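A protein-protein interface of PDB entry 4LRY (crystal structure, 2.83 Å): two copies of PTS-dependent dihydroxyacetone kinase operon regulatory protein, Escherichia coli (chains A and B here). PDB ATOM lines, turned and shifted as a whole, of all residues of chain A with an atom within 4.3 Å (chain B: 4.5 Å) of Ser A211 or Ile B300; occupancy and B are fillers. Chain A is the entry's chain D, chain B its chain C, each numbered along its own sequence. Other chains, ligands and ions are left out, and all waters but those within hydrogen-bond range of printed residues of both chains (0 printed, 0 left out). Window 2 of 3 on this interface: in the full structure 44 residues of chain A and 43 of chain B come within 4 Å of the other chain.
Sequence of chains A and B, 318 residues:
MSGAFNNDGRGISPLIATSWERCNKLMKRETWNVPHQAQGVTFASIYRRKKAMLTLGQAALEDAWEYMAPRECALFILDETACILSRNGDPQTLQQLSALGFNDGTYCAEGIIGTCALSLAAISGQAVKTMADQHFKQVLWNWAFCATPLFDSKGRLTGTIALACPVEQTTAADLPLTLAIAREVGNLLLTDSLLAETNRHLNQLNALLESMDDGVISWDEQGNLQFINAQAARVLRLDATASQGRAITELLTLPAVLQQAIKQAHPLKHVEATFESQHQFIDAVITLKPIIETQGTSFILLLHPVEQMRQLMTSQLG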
ATOM      1  N   ALA A 207      25.864  17.511  20.071  1.00  0.00           N
ATOM      2  CA  ALA A 207      24.979  16.501  20.581  1.00  0.00           C
ATOM      3  C   ALA A 207      23.964  17.109  21.572  1.00  0.00           C
ATOM      4  O   ALA A 207      22.814  16.668  21.619  1.00  0.00           O
ATOM      5  CB  ALA A 207      25.766  15.396  21.216  1.00  0.00           C
ATOM      6  N   LEU A 208      24.345  18.134  22.334  1.00  0.00           N
ATOM      7  CA  LEU A 208      23.386  18.696  23.313  1.00  0.00           C
ATOM      8  C   LEU A 208      22.319  19.529  22.616  1.00  0.00           C
ATOM      9  O   LEU A 208      21.116  19.264  22.775  1.00  0.00           O
ATOM     10  CB  LEU A 208      24.072  19.467  24.441  1.00  0.00           C
ATOM     11  CG  LEU A 208      24.446  18.680  25.718  1.00  0.00           C
ATOM     12  CD1 LEU A 208      24.519  17.157  25.544  1.00  0.00           C
ATOM     13  CD2 LEU A 208      25.731  19.191  26.377  1.00  0.00           C
ATOM     14  N   LEU A 209      22.739  20.499  21.800  1.00  0.00           N
ATOM     15  CA  LEU A 209      21.773  21.260  21.007  1.00  0.00           C
ATOM     16  C   LEU A 209      20.956  20.341  20.068  1.00  0.00           C
ATOM     17  O   LEU A 209      19.766  20.534  19.867  1.00  0.00           O
ATOM     18  CB  LEU A 209      22.466  22.386  20.250  1.00  0.00           C
ATOM     19  CG  LEU A 209      23.111  23.497  21.086  1.00  0.00           C
ATOM     20  CD1 LEU A 209      24.365  23.940  20.388  1.00  0.00           C
ATOM     21  CD2 LEU A 209      22.225  24.686  21.318  1.00  0.00           C
ATOM     22  N   GLU A 210      21.591  19.316  19.523  1.00  0.00           N
ATOM     23  CA  GLU A 210      20.892  18.464  18.576  1.00  0.00           C
ATOM     24  C   GLU A 210      19.776  17.643  19.224  1.00  0.00           C
ATOM     25  O   GLU A 210      18.840  17.223  18.566  1.00  0.00           O
ATOM     26  CB  GLU A 210      21.863  17.563  17.784  1.00  0.00           C
ATOM     27  CG  GLU A 210      21.432  17.330  16.325  1.00  0.00           C
ATOM     28  CD  GLU A 210      21.476  18.630  15.514  1.00  0.00           C
ATOM     29  OE1 GLU A 210      22.586  19.000  15.021  1.00  0.00           O
ATOM     30  OE2 GLU A 210      20.409  19.276  15.392  1.00  0.00           O
ATOM     31  N   SER A 211      19.861  17.399  20.508  1.00  0.00           N
ATOM     32  CA  SER A 211      18.773  16.678  21.125  1.00  0.00           C
ATOM     33  C   SER A 211      18.042  17.545  22.160  1.00  0.00           C
ATOM     34  O   SER A 211      17.586  17.043  23.183  1.00  0.00           O
ATOM     35  CB  SER A 211      19.246  15.343  21.702  1.00  0.00           C
ATOM     36  OG  SER A 211      20.131  15.572  22.763  1.00  0.00           O
ATOM     37  N   MET A 212      17.926  18.847  21.861  1.00  0.00           N
ATOM     38  CA  MET A 212      17.024  19.776  22.563  1.00  0.00           C
ATOM     39  C   MET A 212      15.590  19.340  22.481  1.00  0.00           C
ATOM     40  O   MET A 212      15.294  18.150  22.499  1.00  0.00           O
ATOM     41  CB  MET A 212      17.092  21.172  21.962  1.00  0.00           C
ATOM     42  CG  MET A 212      17.990  22.095  22.683  1.00  0.00           C
ATOM     43  SD  MET A 212      18.333  21.568  24.393  1.00  0.00           S
ATOM     44  CE  MET A 212      19.100  23.033  25.048  1.00  0.00           C
ATOM     45  N   VAL B 216      20.101  23.199  31.553  1.00  0.00           N
ATOM     46  CA  VAL B 216      20.658  22.011  30.939  1.00  0.00           C
ATOM     47  C   VAL B 216      21.922  21.500  31.643  1.00  0.00           C
ATOM     48  O   VAL B 216      22.823  22.270  31.995  1.00  0.00           O
ATOM     49  CB  VAL B 216      20.848  22.206  29.402  1.00  0.00           C
ATOM     50  CG1 VAL B 216      20.905  23.690  29.031  1.00  0.00           C
ATOM     51  CG2 VAL B 216      22.047  21.414  28.896  1.00  0.00           C
ATOM     52  N   ILE B 217      21.941  20.195  31.888  1.00  0.00           N
ATOM     53  CA  ILE B 217      23.072  19.528  32.492  1.00  0.00           C
ATOM     54  C   ILE B 217      23.294  18.295  31.652  1.00  0.00           C
ATOM     55  O   ILE B 217      22.326  17.610  31.315  1.00  0.00           O
ATOM     56  CB  ILE B 217      22.762  19.079  33.922  1.00  0.00           C
ATOM     57  CG1 ILE B 217      22.874  20.258  34.873  1.00  0.00           C
ATOM     58  CG2 ILE B 217      23.756  18.020  34.393  1.00  0.00           C
ATOM     59  CD1 ILE B 217      22.583  19.895  36.330  1.00  0.00           C
ATOM     60  N   SER B 218      24.545  18.012  31.289  1.00  0.00           N
ATOM     61  CA  SER B 218      24.851  16.735  30.631  1.00  0.00           C
ATOM     62  C   SER B 218      25.871  15.933  31.425  1.00  0.00           C
ATOM     63  O   SER B 218      26.623  16.506  32.237  1.00  0.00           O
ATOM     64  CB  SER B 218      25.325  16.944  29.192  1.00  0.00           C
ATOM     65  OG  SER B 218      26.538  17.676  29.130  1.00  0.00           O
ATOM     66  N   THR B 287      13.029  16.886  31.795  1.00  0.00           N
ATOM     67  CA  THR B 287      13.028  15.888  30.727  1.00  0.00           C
ATOM     68  C   THR B 287      14.417  15.303  30.653  1.00  0.00           C
ATOM     69  O   THR B 287      15.414  16.032  30.795  1.00  0.00           O
ATOM     70  CB  THR B 287      12.643  16.488  29.397  1.00  0.00           C
ATOM     71  OG1 THR B 287      11.334  17.047  29.505  1.00  0.00           O
ATOM     72  CG2 THR B 287      12.631  15.434  28.308  1.00  0.00           C
ATOM     73  N   LEU B 288      14.488  13.987  30.465  1.00  0.00           N
ATOM     74  CA  LEU B 288      15.784  13.297  30.484  1.00  0.00           C
ATOM     75  C   LEU B 288      15.988  12.461  29.228  1.00  0.00           C
ATOM     76  O   LEU B 288      15.149  11.620  28.892  1.00  0.00           O
ATOM     77  CB  LEU B 288      15.965  12.427  31.745  1.00  0.00           C
ATOM     78  CG  LEU B 288      17.305  11.658  31.822  1.00  0.00           C
ATOM     79  CD1 LEU B 288      18.393  12.464  32.536  1.00  0.00           C
ATOM     80  CD2 LEU B 288      17.171  10.277  32.464  1.00  0.00           C
ATOM     81  N   LYS B 289      17.116  12.682  28.553  1.00  0.00           N
ATOM     82  CA  LYS B 289      17.349  12.035  27.271  1.00  0.00           C
ATOM     83  C   LYS B 289      18.685  11.254  27.155  1.00  0.00           C
ATOM     84  O   LYS B 289      19.770  11.828  27.361  1.00  0.00           O
ATOM     85  CB  LYS B 289      17.173  13.055  26.141  1.00  0.00           C
ATOM     86  CG  LYS B 289      16.142  12.628  25.081  1.00  0.00           C
ATOM     87  CD  LYS B 289      14.981  13.593  24.939  1.00  0.00           C
ATOM     88  CE  LYS B 289      15.491  14.976  24.554  1.00  0.00           C
ATOM     89  NZ  LYS B 289      14.504  15.742  23.761  1.00  0.00           N
ATOM     90  N   ILE B 291      21.754   9.582  25.248  1.00  0.00           N
ATOM     91  CA  ILE B 291      22.522   9.982  24.084  1.00  0.00           C
ATOM     92  C   ILE B 291      23.404   8.792  23.676  1.00  0.00           C
ATOM     93  O   ILE B 291      24.555   8.726  24.075  1.00  0.00           O
ATOM     94  CB  ILE B 291      23.317  11.295  24.382  1.00  0.00           C
ATOM     95  CG1 ILE B 291      22.332  12.474  24.525  1.00  0.00           C
ATOM     96  CG2 ILE B 291      24.370  11.558  23.311  1.00  0.00           C
ATOM     97  CD1 ILE B 291      22.914  13.879  24.468  1.00  0.00           C
ATOM     98  N   PHE B 299      23.783  11.647  28.931  1.00  0.00           N
ATOM     99  CA  PHE B 299      22.436  12.147  29.202  1.00  0.00           C
ATOM    100  C   PHE B 299      22.404  13.649  29.172  1.00  0.00           C
ATOM    101  O   PHE B 299      23.388  14.292  29.580  1.00  0.00           O
ATOM    102  CB  PHE B 299      21.919  11.676  30.577  1.00  0.00           C
ATOM    103  CG  PHE B 299      21.784  10.181  30.703  1.00  0.00           C
ATOM    104  CD1 PHE B 299      20.629   9.529  30.267  1.00  0.00           C
ATOM    105  CD2 PHE B 299      22.821   9.418  31.241  1.00  0.00           C
ATOM    106  CE1 PHE B 299      20.510   8.140  30.377  1.00  0.00           C
ATOM    107  CE2 PHE B 299      22.714   8.034  31.355  1.00  0.00           C
ATOM    108  CZ  PHE B 299      21.553   7.394  30.923  1.00  0.00           C
ATOM    109  N   ILE B 300      21.290  14.199  28.673  1.00  0.00           N
ATOM    110  CA  ILE B 300      20.893  15.562  29.013  1.00  0.00           C
ATOM    111  C   ILE B 300      19.763  15.453  29.998  1.00  0.00           C
ATOM    112  O   ILE B 300      18.906  14.562  29.896  1.00  0.00           O
ATOM    113  CB  ILE B 300      20.226  16.380  27.887  1.00  0.00           C
ATOM    114  CG1 ILE B 300      20.700  16.036  26.508  1.00  0.00           C
ATOM    115  CG2 ILE B 300      20.398  17.894  28.108  1.00  0.00           C
ATOM    116  CD1 ILE B 300      20.008  16.983  25.522  1.00  0.00           C
ATOM    117  N   LEU B 301      19.745  16.420  30.906  1.00  0.00           N
ATOM    118  CA  LEU B 301      18.656  16.669  31.806  1.00  0.00           C
ATOM    119  C   LEU B 301      18.265  18.096  31.537  1.00  0.00           C
ATOM    120  O   LEU B 301      19.084  19.014  31.615  1.00  0.00           O
ATOM    121  CB  LEU B 301      19.140  16.538  33.247  1.00  0.00           C
ATOM    122  CG  LEU B 301      18.130  16.787  34.365  1.00  0.00           C
ATOM    123  CD1 LEU B 301      17.441  15.521  34.726  1.00  0.00           C
ATOM    124  CD2 LEU B 301      18.849  17.349  35.553  1.00  0.00           C
ATOM    125  N   LEU B 302      17.000  18.289  31.212  1.00  0.00           N
ATOM    126  CA  LEU B 302      16.476  19.638  31.103  1.00  0.00           C
ATOM    127  C   LEU B 302      15.638  19.980  32.311  1.00  0.00           C
ATOM    128  O   LEU B 302      14.706  19.239  32.688  1.00  0.00           O
ATOM    129  CB  LEU B 302      15.673  19.816  29.823  1.00  0.00           C
ATOM    130  CG  LEU B 302      16.499  19.648  28.553  1.00  0.00           C
ATOM    131  CD1 LEU B 302      16.156  18.323  27.944  1.00  0.00           C
ATOM    132  CD2 LEU B 302      16.143  20.767  27.605  1.00  0.00           C
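Glu A210 touches none of the printed residues of chain B. Ser A211 touches just these residues of chain B: Lys B289 (3.2 Å), Ile B291 (3.7 Å) and Ile B300 (3.1 Å). Printed residues of chain B within 4 Å of Met A212: Lys B289 and Leu B302. Of the printed residues of chain A, Ser B218 touches Leu A208. Of the printed residues of chain A, Ile B300 touches Leu A208 and Ser A211. Leu B301 touches none of the printed residues of chain A. The nearest printed residue of chain A that does not touch Ile B300 is Met A212 (4.6 Å).
No position is printed for both chains. Of the 9 pairs that touch across the chains among the printed residues, none has its exchanged pair printed and touching as well.
The side-chain amino group (NZ) of Lys B289 sits close to the backbone carbonyl oxygen (O) of Ser A211. The side-chain amino group (NZ) of Lys B289 lies within hydrogen-bond range of the backbone carbonyl oxygen (O) of Met A212 (2.8 Å).
Among the printed residues, merely in contact across the chains: Ala A207 with Ile B291 (3.99 Å), Leu A208 with Ser B218 (3.2 Å), Leu A208 with Ile B291 (3.8 Å), Leu A208 with Ile B300 (3.7 Å), Ser A211 with Ile B291 (3.7 Å), Ser A211 with Ile B300 (3.1 Å) and Met A212 with Leu B302 (3.97 Å).
Printed residues of chain A that touch a printed residue of chain B: Ala A207, Leu A208, Ser A211 and Met A212. Along chain A the printed residues that touch a printed residue of chain B span positions 207 to 212. Of the 11 printed residues of chain B, 5 touch a printed residue of chain A. Hydrophobic or aromatic side chains of chain B that line the printed part of chain A: Ile B291, Ile B300 and Leu B302. Among the printed residues, no Asp or Glu carboxylate lies within 4 Å of a Lys or Arg side-chain nitrogen of the other chain.
The backbone carbonyl oxygen (O) of Thr B287 is in hydrogen-bond range of the backbone NH (N) of Leu B302 (2.8 Å). N of Lys B289 is in hydrogen-bond range of O of Ile B300. O of Ala A207 lies within hydrogen-bond range of OG of Ser A211, at 3.1 Å.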
